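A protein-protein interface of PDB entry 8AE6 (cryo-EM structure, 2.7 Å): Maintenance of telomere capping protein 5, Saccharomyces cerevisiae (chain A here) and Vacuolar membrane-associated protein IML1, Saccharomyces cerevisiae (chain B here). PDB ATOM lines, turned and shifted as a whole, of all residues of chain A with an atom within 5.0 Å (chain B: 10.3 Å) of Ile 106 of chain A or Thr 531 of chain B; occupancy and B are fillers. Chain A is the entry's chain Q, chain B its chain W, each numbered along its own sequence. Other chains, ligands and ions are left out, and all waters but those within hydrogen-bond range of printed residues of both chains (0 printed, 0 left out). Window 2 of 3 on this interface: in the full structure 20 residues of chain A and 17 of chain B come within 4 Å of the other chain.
Of the 15 printed residues of chain B, 5 touch a printed residue of chain A.
Hydrophobic or aromatic side chains of chain A that line the printed part of chain B: His 64, Ile 94, Ile 106, Val 109 and His 111.
O of Gly 529 of chain B is in hydrogen-bond range of NE2 of His 111 of chain A (2.7 Å).
OD1 of Asn 104 of chain A sits at hydrogen-bond distance from ND2 of Asn 533 of chain B (2.6 Å).
The side-chain amino group (NZ) of Lys 92 of chain A is in hydrogen-bond range of the backbone carbonyl oxygen (O) of Met 528 of chain B.
Of the printed residues of chain B, His 64 of chain A touches Thr 531.
Asn 104 of chain A touches just one residue of chain B: Asn 533.
No residue of chain B comes within 4 Å of Ala 105 of chain A.
Of chain B, only Thr 531 and Asn 533 come within 4 Å of Ile 106 of chain A.
Of the printed residues of chain B, His 111 of chain A touches Gly 529 and Glu 534.
Of the printed residues of chain A, Met 528 of chain B touches Lys 92 (3.2 Å).
Of the printed residues of chain A, Gly 529 of chain B touches Lys 92 and His 111.
Of chain A, only His 64, Lys 92, Ile 94, Ile 106 and Val 109 come within 4 Å of Thr 531 of chain B.
The nearest printed residue of chain B that does not touch His 64 of chain A is Glu 532 of chain B (4.6 Å).
The backbone carbonyl oxygen (O) of Asp 524 of chain B sits at hydrogen-bond distance from the backbone NH (N) of Gly 529 of chain B.
The backbone carbonyl oxygen (O) of Val 109 of chain A is in hydrogen-bond range of a ring nitrogen (ND1) of His 111 of chain A, 3.5 Å away.
His 64 of chain A touches Thr 531 of chain B (CE1 to CG2, 3.9 Å).
Lys 92 of chain A touches Gly 529 of chain B.
Lys 92 of chain A touches Thr 531 of chain B (CE to OG1, 3.3 Å).
Thr 531 of chain B touches Ile 94 of chain A (CG2 to CD1, 3.96 Å).
Thr 531 of chain B touches Ile 106 of chain A (CG2 to CD1, 3.7 Å).
Asn 533 of chain B touches Ile 106 of chain A (ND2 to CD1, 3.5 Å).
Val 109 of chain A touches Thr 531 of chain B (CG2 to OG1, 3.3 Å).
His 111 of chain A touches Glu 534 of chain B (CE1 to OE2, 3.3 Å).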
ATOM      1  N   HIS A  64      -3.783  -3.449  16.546  1.00  0.00           N
ATOM      2  CA  HIS A  64      -3.544  -3.270  15.116  1.00  0.00           C
ATOM      3  C   HIS A  64      -2.361  -4.151  14.749  1.00  0.00           C
ATOM      4  O   HIS A  64      -1.220  -3.824  15.087  1.00  0.00           O
ATOM      5  CB  HIS A  64      -3.274  -1.818  14.756  1.00  0.00           C
ATOM      6  CG  HIS A  64      -3.083  -1.597  13.290  1.00  0.00           C
ATOM      7  ND1 HIS A  64      -4.094  -1.778  12.375  1.00  0.00           N
ATOM      8  CD2 HIS A  64      -1.993  -1.223  12.577  1.00  0.00           C
ATOM      9  CE1 HIS A  64      -3.641  -1.523  11.161  1.00  0.00           C
ATOM     10  NE2 HIS A  64      -2.367  -1.186  11.257  1.00  0.00           N
ATOM     11  N   LYS A  92       0.994   3.888   5.968  1.00  0.00           N
ATOM     12  CA  LYS A  92      -0.116   4.741   6.356  1.00  0.00           C
ATOM     13  C   LYS A  92      -0.006   5.102   7.827  1.00  0.00           C
ATOM     14  O   LYS A  92       0.503   4.327   8.640  1.00  0.00           O
ATOM     15  CB  LYS A  92      -1.463   4.066   6.072  1.00  0.00           C
ATOM     16  CG  LYS A  92      -1.647   2.719   6.740  1.00  0.00           C
ATOM     17  CD  LYS A  92      -2.538   1.813   5.919  1.00  0.00           C
ATOM     18  CE  LYS A  92      -2.856   0.536   6.673  1.00  0.00           C
ATOM     19  NZ  LYS A  92      -1.628  -0.227   7.018  1.00  0.00           N
ATOM     20  N   ILE A  94      -1.969   6.161  11.314  1.00  0.00           N
ATOM     21  CA  ILE A  94      -3.241   5.833  11.939  1.00  0.00           C
ATOM     22  C   ILE A  94      -3.472   6.795  13.095  1.00  0.00           C
ATOM     23  O   ILE A  94      -2.640   6.892  14.005  1.00  0.00           O
ATOM     24  CB  ILE A  94      -3.268   4.375  12.417  1.00  0.00           C
ATOM     25  CG1 ILE A  94      -3.329   3.428  11.218  1.00  0.00           C
ATOM     26  CG2 ILE A  94      -4.432   4.140  13.363  1.00  0.00           C
ATOM     27  CD1 ILE A  94      -3.520   1.985  11.588  1.00  0.00           C
ATOM     28  N   ILE A  95      -4.597   7.499  13.062  1.00  0.00           N
ATOM     29  CA  ILE A  95      -5.000   8.399  14.137  1.00  0.00           C
ATOM     30  C   ILE A  95      -5.936   7.642  15.066  1.00  0.00           C
ATOM     31  O   ILE A  95      -7.015   7.199  14.654  1.00  0.00           O
ATOM     32  CB  ILE A  95      -5.655   9.685  13.606  1.00  0.00           C
ATOM     33  CG1 ILE A  95      -4.652  10.534  12.812  1.00  0.00           C
ATOM     34  CG2 ILE A  95      -6.240  10.492  14.747  1.00  0.00           C
ATOM     35  CD1 ILE A  95      -4.575  10.249  11.337  1.00  0.00           C
ATOM     36  N   TRP A  96      -5.520   7.491  16.315  1.00  0.00           N
ATOM     37  CA  TRP A  96      -6.256   6.723  17.306  1.00  0.00           C
ATOM     38  C   TRP A  96      -7.113   7.651  18.150  1.00  0.00           C
ATOM     39  O   TRP A  96      -6.665   8.721  18.564  1.00  0.00           O
ATOM     40  CB  TRP A  96      -5.304   5.944  18.215  1.00  0.00           C
ATOM     41  CG  TRP A  96      -4.412   4.989  17.508  1.00  0.00           C
ATOM     42  CD1 TRP A  96      -3.251   5.280  16.859  1.00  0.00           C
ATOM     43  CD2 TRP A  96      -4.595   3.577  17.385  1.00  0.00           C
ATOM     44  NE1 TRP A  96      -2.701   4.138  16.337  1.00  0.00           N
ATOM     45  CE2 TRP A  96      -3.508   3.078  16.647  1.00  0.00           C
ATOM     46  CE3 TRP A  96      -5.577   2.687  17.824  1.00  0.00           C
ATOM     47  CZ2 TRP A  96      -3.376   1.730  16.338  1.00  0.00           C
ATOM     48  CZ3 TRP A  96      -5.444   1.354  17.515  1.00  0.00           C
ATOM     49  CH2 TRP A  96      -4.352   0.886  16.784  1.00  0.00           C
ATOM     50  N   ASN A  97      -8.345   7.235  18.401  1.00  0.00           N
ATOM     51  CA  ASN A  97      -9.259   7.953  19.279  1.00  0.00           C
ATOM     52  C   ASN A  97      -9.383   7.153  20.567  1.00  0.00           C
ATOM     53  O   ASN A  97     -10.012   6.090  20.588  1.00  0.00           O
ATOM     54  CB  ASN A  97     -10.619   8.144  18.611  1.00  0.00           C
ATOM     55  CG  ASN A  97     -11.398   9.302  19.198  1.00  0.00           C
ATOM     56  OD1 ASN A  97     -11.094   9.780  20.288  1.00  0.00           O
ATOM     57  ND2 ASN A  97     -12.419   9.750  18.481  1.00  0.00           N
ATOM     58  N   LYS A 100     -12.804   6.355  22.021  1.00  0.00           N
ATOM     59  CA  LYS A 100     -13.445   5.178  21.463  1.00  0.00           C
ATOM     60  C   LYS A 100     -12.996   3.927  22.212  1.00  0.00           C
ATOM     61  O   LYS A 100     -11.997   3.928  22.935  1.00  0.00           O
ATOM     62  CB  LYS A 100     -13.111   5.046  19.976  1.00  0.00           C
ATOM     63  CG  LYS A 100     -13.909   5.968  19.073  1.00  0.00           C
ATOM     64  CD  LYS A 100     -13.620   5.676  17.612  1.00  0.00           C
ATOM     65  CE  LYS A 100     -14.381   6.617  16.695  1.00  0.00           C
ATOM     66  NZ  LYS A 100     -14.168   6.273  15.261  1.00  0.00           N
ATOM     67  N   ASN A 104     -12.436  -0.863  18.460  1.00  0.00           N
ATOM     68  CA  ASN A 104     -12.360   0.040  17.312  1.00  0.00           C
ATOM     69  C   ASN A 104     -11.972   1.416  17.842  1.00  0.00           C
ATOM     70  O   ASN A 104     -12.836   2.242  18.140  1.00  0.00           O
ATOM     71  CB  ASN A 104     -13.681   0.075  16.552  1.00  0.00           C
ATOM     72  CG  ASN A 104     -13.502   0.436  15.094  1.00  0.00           C
ATOM     73  OD1 ASN A 104     -12.402   0.781  14.660  1.00  0.00           O
ATOM     74  ND2 ASN A 104     -14.582   0.359  14.328  1.00  0.00           N
ATOM     75  N   ALA A 105     -10.665   1.655  17.956  1.00  0.00           N
ATOM     76  CA  ALA A 105     -10.142   2.928  18.433  1.00  0.00           C
ATOM     77  C   ALA A 105      -9.577   3.793  17.318  1.00  0.00           C
ATOM     78  O   ALA A 105      -9.136   4.914  17.589  1.00  0.00           O
ATOM     79  CB  ALA A 105      -9.056   2.693  19.490  1.00  0.00           C
ATOM     80  N   ILE A 106      -9.578   3.304  16.085  1.00  0.00           N
ATOM     81  CA  ILE A 106      -9.025   4.046  14.961  1.00  0.00           C
ATOM     82  C   ILE A 106     -10.088   5.002  14.438  1.00  0.00           C
ATOM     83  O   ILE A 106     -11.199   4.585  14.094  1.00  0.00           O
ATOM     84  CB  ILE A 106      -8.544   3.093  13.860  1.00  0.00           C
ATOM     85  CG1 ILE A 106      -7.428   2.201  14.401  1.00  0.00           C
ATOM     86  CG2 ILE A 106      -8.085   3.869  12.641  1.00  0.00           C
ATOM     87  CD1 ILE A 106      -6.905   1.203  13.412  1.00  0.00           C
ATOM     88  N   GLU A 107      -9.751   6.290  14.378  1.00  0.00           N
ATOM     89  CA  GLU A 107     -10.681   7.295  13.880  1.00  0.00           C
ATOM     90  C   GLU A 107     -10.562   7.456  12.367  1.00  0.00           C
ATOM     91  O   GLU A 107     -11.537   7.250  11.638  1.00  0.00           O
ATOM     92  CB  GLU A 107     -10.444   8.630  14.593  1.00  0.00           C
ATOM     93  CG  GLU A 107     -11.637   9.564  14.559  1.00  0.00           C
ATOM     94  CD  GLU A 107     -11.504  10.712  15.538  1.00  0.00           C
ATOM     95  OE1 GLU A 107     -10.514  10.732  16.296  1.00  0.00           O
ATOM     96  OE2 GLU A 107     -12.389  11.593  15.547  1.00  0.00           O
ATOM     97  N   PHE A 108      -9.378   7.820  11.885  1.00  0.00           N
ATOM     98  CA  PHE A 108      -9.141   7.889  10.450  1.00  0.00           C
ATOM     99  C   PHE A 108      -7.671   7.611  10.174  1.00  0.00           C
ATOM    100  O   PHE A 108      -6.814   7.756  11.048  1.00  0.00           O
ATOM    101  CB  PHE A 108      -9.564   9.239   9.856  1.00  0.00           C
ATOM    102  CG  PHE A 108      -9.231  10.424  10.715  1.00  0.00           C
ATOM    103  CD1 PHE A 108      -7.991  11.025  10.634  1.00  0.00           C
ATOM    104  CD2 PHE A 108     -10.171  10.954  11.582  1.00  0.00           C
ATOM    105  CE1 PHE A 108      -7.681  12.119  11.413  1.00  0.00           C
ATOM    106  CE2 PHE A 108      -9.869  12.049  12.369  1.00  0.00           C
ATOM    107  CZ  PHE A 108      -8.622  12.632  12.281  1.00  0.00           C
ATOM    108  N   VAL A 109      -7.397   7.201   8.939  1.00  0.00           N
ATOM    109  CA  VAL A 109      -6.071   6.773   8.511  1.00  0.00           C
ATOM    110  C   VAL A 109      -5.633   7.654   7.350  1.00  0.00           C
ATOM    111  O   VAL A 109      -6.397   7.859   6.399  1.00  0.00           O
ATOM    112  CB  VAL A 109      -6.064   5.289   8.101  1.00  0.00           C
ATOM    113  CG1 VAL A 109      -4.660   4.836   7.753  1.00  0.00           C
ATOM    114  CG2 VAL A 109      -6.636   4.423   9.210  1.00  0.00           C
ATOM    115  N   HIS A 111      -3.750   8.001   4.109  1.00  0.00           N
ATOM    116  CA  HIS A 111      -3.265   7.130   3.042  1.00  0.00           C
ATOM    117  C   HIS A 111      -2.438   7.986   2.089  1.00  0.00           C
ATOM    118  O   HIS A 111      -2.945   8.540   1.114  1.00  0.00           O
ATOM    119  CB  HIS A 111      -4.427   6.441   2.341  1.00  0.00           C
ATOM    120  CG  HIS A 111      -4.923   5.228   3.060  1.00  0.00           C
ATOM    121  ND1 HIS A 111      -5.833   5.295   4.095  1.00  0.00           N
ATOM    122  CD2 HIS A 111      -4.630   3.917   2.902  1.00  0.00           C
ATOM    123  CE1 HIS A 111      -6.082   4.077   4.539  1.00  0.00           C
ATOM    124  NE2 HIS A 111      -5.365   3.222   3.834  1.00  0.00           N
ATOM    125  N   LYS B 340      -9.305   3.538  -8.863  1.00  0.00           N
ATOM    126  CA  LYS B 340     -10.357   2.570  -8.582  1.00  0.00           C
ATOM    127  C   LYS B 340     -11.664   2.922  -9.272  1.00  0.00           C
ATOM    128  O   LYS B 340     -12.491   2.033  -9.498  1.00  0.00           O
ATOM    129  CB  LYS B 340     -10.584   2.464  -7.075  1.00  0.00           C
ATOM    130  CG  LYS B 340      -9.327   2.185  -6.274  1.00  0.00           C
ATOM    131  CD  LYS B 340      -9.667   1.687  -4.884  1.00  0.00           C
ATOM    132  CE  LYS B 340      -8.519   0.892  -4.296  1.00  0.00           C
ATOM    133  NZ  LYS B 340      -8.892   0.251  -3.007  1.00  0.00           N
ATOM    134  N   ASP B 524      -3.910  -4.239  -2.621  1.00  0.00           N
ATOM    135  CA  ASP B 524      -4.288  -3.672  -1.335  1.00  0.00           C
ATOM    136  C   ASP B 524      -4.238  -4.691  -0.207  1.00  0.00           C
ATOM    137  O   ASP B 524      -4.190  -4.298   0.963  1.00  0.00           O
ATOM    138  CB  ASP B 524      -5.686  -3.064  -1.427  1.00  0.00           C
ATOM    139  CG  ASP B 524      -5.717  -1.803  -2.264  1.00  0.00           C
ATOM    140  OD1 ASP B 524      -4.676  -1.458  -2.860  1.00  0.00           O
ATOM    141  OD2 ASP B 524      -6.783  -1.159  -2.326  1.00  0.00           O
ATOM    142  N   LEU B 525      -4.247  -5.983  -0.523  1.00  0.00           N
ATOM    143  CA  LEU B 525      -4.107  -7.017   0.491  1.00  0.00           C
ATOM    144  C   LEU B 525      -2.683  -7.530   0.625  1.00  0.00           C
ATOM    145  O   LEU B 525      -2.288  -7.944   1.718  1.00  0.00           O
ATOM    146  CB  LEU B 525      -5.038  -8.195   0.184  1.00  0.00           C
ATOM    147  CG  LEU B 525      -6.517  -7.932   0.457  1.00  0.00           C
ATOM    148  CD1 LEU B 525      -7.369  -9.021  -0.154  1.00  0.00           C
ATOM    149  CD2 LEU B 525      -6.768  -7.819   1.949  1.00  0.00           C
ATOM    150  N   MET B 527       0.012  -5.510   0.066  1.00  0.00           N
ATOM    151  CA  MET B 527       0.668  -4.398   0.740  1.00  0.00           C
ATOM    152  C   MET B 527      -0.005  -4.013   2.046  1.00  0.00           C
ATOM    153  O   MET B 527       0.529  -3.153   2.756  1.00  0.00           O
ATOM    154  CB  MET B 527       0.715  -3.175  -0.179  1.00  0.00           C
ATOM    155  CG  MET B 527       1.434  -3.407  -1.492  1.00  0.00           C
ATOM    156  SD  MET B 527       3.211  -3.598  -1.296  1.00  0.00           S
ATOM    157  CE  MET B 527       3.744  -1.894  -1.364  1.00  0.00           C
ATOM    158  N   MET B 528      -1.142  -4.639   2.371  1.00  0.00           N
ATOM    159  CA  MET B 528      -1.967  -4.310   3.539  1.00  0.00           C
ATOM    160  C   MET B 528      -2.333  -2.827   3.560  1.00  0.00           C
ATOM    161  O   MET B 528      -2.255  -2.156   4.590  1.00  0.00           O
ATOM    162  CB  MET B 528      -1.283  -4.730   4.842  1.00  0.00           C
ATOM    163  CG  MET B 528      -1.294  -6.228   5.084  1.00  0.00           C
ATOM    164  SD  MET B 528      -1.191  -6.652   6.830  1.00  0.00           S
ATOM    165  CE  MET B 528      -1.115  -8.439   6.741  1.00  0.00           C
ATOM    166  N   GLY B 529      -2.737  -2.314   2.396  1.00  0.00           N
ATOM    167  CA  GLY B 529      -3.021  -0.899   2.257  1.00  0.00           C
ATOM    168  C   GLY B 529      -4.329  -0.449   2.860  1.00  0.00           C
ATOM    169  O   GLY B 529      -4.543   0.758   3.014  1.00  0.00           O
ATOM    170  N   ILE B 530      -5.211  -1.381   3.202  1.00  0.00           N
ATOM    171  CA  ILE B 530      -6.506  -1.057   3.786  1.00  0.00           C
ATOM    172  C   ILE B 530      -6.472  -1.442   5.260  1.00  0.00           C
ATOM    173  O   ILE B 530      -6.173  -2.592   5.604  1.00  0.00           O
ATOM    174  CB  ILE B 530      -7.649  -1.768   3.047  1.00  0.00           C
ATOM    175  CG1 ILE B 530      -7.439  -1.683   1.536  1.00  0.00           C
ATOM    176  CG2 ILE B 530      -8.979  -1.148   3.416  1.00  0.00           C
ATOM    177  CD1 ILE B 530      -7.551  -0.277   0.973  1.00  0.00           C
ATOM    178  N   THR B 531      -6.768  -0.476   6.123  1.00  0.00           N
ATOM    179  CA  THR B 531      -6.747  -0.688   7.562  1.00  0.00           C
ATOM    180  C   THR B 531      -7.879  -1.627   7.964  1.00  0.00           C
ATOM    181  O   THR B 531      -8.979  -1.568   7.412  1.00  0.00           O
ATOM    182  CB  THR B 531      -6.863   0.661   8.281  1.00  0.00           C
ATOM    183  OG1 THR B 531      -5.822   1.530   7.818  1.00  0.00           O
ATOM    184  CG2 THR B 531      -6.718   0.515   9.784  1.00  0.00           C
ATOM    185  N   GLU B 532      -7.592  -2.499   8.946  1.00  0.00           N
ATOM    186  CA  GLU B 532      -8.469  -3.620   9.288  1.00  0.00           C
ATOM    187  C   GLU B 532      -9.860  -3.171   9.720  1.00  0.00           C
ATOM    188  O   GLU B 532     -10.835  -3.904   9.518  1.00  0.00           O
ATOM    189  CB  GLU B 532      -7.823  -4.452  10.396  1.00  0.00           C
ATOM    190  CG  GLU B 532      -8.415  -5.841  10.578  1.00  0.00           C
ATOM    191  CD  GLU B 532      -7.705  -6.640  11.652  1.00  0.00           C
ATOM    192  OE1 GLU B 532      -6.830  -6.070  12.336  1.00  0.00           O
ATOM    193  OE2 GLU B 532      -8.022  -7.836  11.815  1.00  0.00           O
ATOM    194  N   ASN B 533      -9.982  -1.975  10.285  1.00  0.00           N
ATOM    195  CA  ASN B 533     -11.281  -1.490  10.737  1.00  0.00           C
ATOM    196  C   ASN B 533     -12.141  -0.924   9.615  1.00  0.00           C
ATOM    197  O   ASN B 533     -13.316  -0.635   9.855  1.00  0.00           O
ATOM    198  CB  ASN B 533     -11.095  -0.422  11.818  1.00  0.00           C
ATOM    199  CG  ASN B 533     -10.264  -0.915  12.986  1.00  0.00           C
ATOM    200  OD1 ASN B 533      -9.793  -2.051  12.993  1.00  0.00           O
ATOM    201  ND2 ASN B 533     -10.087  -0.060  13.988  1.00  0.00           N
ATOM    202  N   GLU B 534     -11.604  -0.752   8.406  1.00  0.00           N
ATOM    203  CA  GLU B 534     -12.349  -0.083   7.349  1.00  0.00           C
ATOM    204  C   GLU B 534     -12.625  -0.945   6.124  1.00  0.00           C
ATOM    205  O   GLU B 534     -13.234  -0.447   5.170  1.00  0.00           O
ATOM    206  CB  GLU B 534     -11.633   1.206   6.920  1.00  0.00           C
ATOM    207  CG  GLU B 534     -10.402   1.007   6.060  1.00  0.00           C
ATOM    208  CD  GLU B 534      -9.912   2.297   5.432  1.00  0.00           C
ATOM    209  OE1 GLU B 534     -10.618   3.322   5.545  1.00  0.00           O
ATOM    210  OE2 GLU B 534      -8.821   2.286   4.826  1.00  0.00           O
ATOM    211  N   LEU B 535     -12.214  -2.215   6.110  1.00  0.00           N
ATOM    212  CA  LEU B 535     -12.670  -3.131   5.067  1.00  0.00           C
ATOM    213  C   LEU B 535     -13.531  -4.252   5.646  1.00  0.00           C
ATOM    214  O   LEU B 535     -13.687  -5.298   5.013  1.00  0.00           O
ATOM    215  CB  LEU B 535     -11.500  -3.709   4.259  1.00  0.00           C
ATOM    216  CG  LEU B 535     -10.494  -4.766   4.734  1.00  0.00           C
ATOM    217  CD1 LEU B 535      -9.753  -5.321   3.532  1.00  0.00           C
ATOM    218  CD2 LEU B 535      -9.512  -4.255   5.744  1.00  0.00           C
ATOM    219  N   ILE B 536     -14.093  -4.038   6.839  1.00  0.00           N
ATOM    220  CA  ILE B 536     -15.023  -4.997   7.427  1.00  0.00           C
ATOM    221  C   ILE B 536     -16.262  -5.110   6.544  1.00  0.00           C
ATOM    222  O   ILE B 536     -16.742  -4.116   5.985  1.00  0.00           O
ATOM    223  CB  ILE B 536     -15.372  -4.564   8.863  1.00  0.00           C
ATOM    224  CG1 ILE B 536     -14.104  -4.501   9.717  1.00  0.00           C
ATOM    225  CG2 ILE B 536     -16.384  -5.502   9.517  1.00  0.00           C
ATOM    226  CD1 ILE B 536     -13.482  -5.859   9.997  1.00  0.00           C
ATOM    227  N   ARG B 537     -16.752  -6.345   6.387  1.00  0.00           N
ATOM    228  CA  ARG B 537     -17.854  -6.645   5.482  1.00  0.00           C
ATOM    229  C   ARG B 537     -19.124  -5.894   5.870  1.00  0.00           C
ATOM    230  O   ARG B 537     -19.526  -5.887   7.038  1.00  0.00           O
ATOM    231  CB  ARG B 537     -18.107  -8.154   5.480  1.00  0.00           C
ATOM    232  CG  ARG B 537     -19.517  -8.566   5.117  1.00  0.00           C
ATOM    233  CD  ARG B 537     -19.635 -10.065   4.928  1.00  0.00           C
ATOM    234  NE  ARG B 537     -19.389 -10.791   6.169  1.00  0.00           N
ATOM    235  CZ  ARG B 537     -20.295 -11.530   6.797  1.00  0.00           C
ATOM    236  NH1 ARG B 537     -21.524 -11.666   6.326  1.00  0.00           N
ATOM    237  NH2 ARG B 537     -19.959 -12.148   7.925  1.00  0.00           N
ATOM    238  N   GLU B 538     -19.748  -5.253   4.880  1.00  0.00           N
ATOM    239  CA  GLU B 538     -20.965  -4.479   5.083  1.00  0.00           C
ATOM    240  C   GLU B 538     -22.216  -5.203   4.599  1.00  0.00           C
ATOM    241  O   GLU B 538     -23.241  -5.182   5.288  1.00  0.00           O
ATOM    242  CB  GLU B 538     -20.857  -3.126   4.377  1.00  0.00           C
ATOM    243  CG  GLU B 538     -19.664  -2.291   4.812  1.00  0.00           C
ATOM    244  CD  GLU B 538     -19.859  -1.660   6.178  1.00  0.00           C
ATOM    245  OE1 GLU B 538     -21.019  -1.378   6.545  1.00  0.00           O
ATOM    246  OE2 GLU B 538     -18.852  -1.444   6.882  1.00  0.00           O
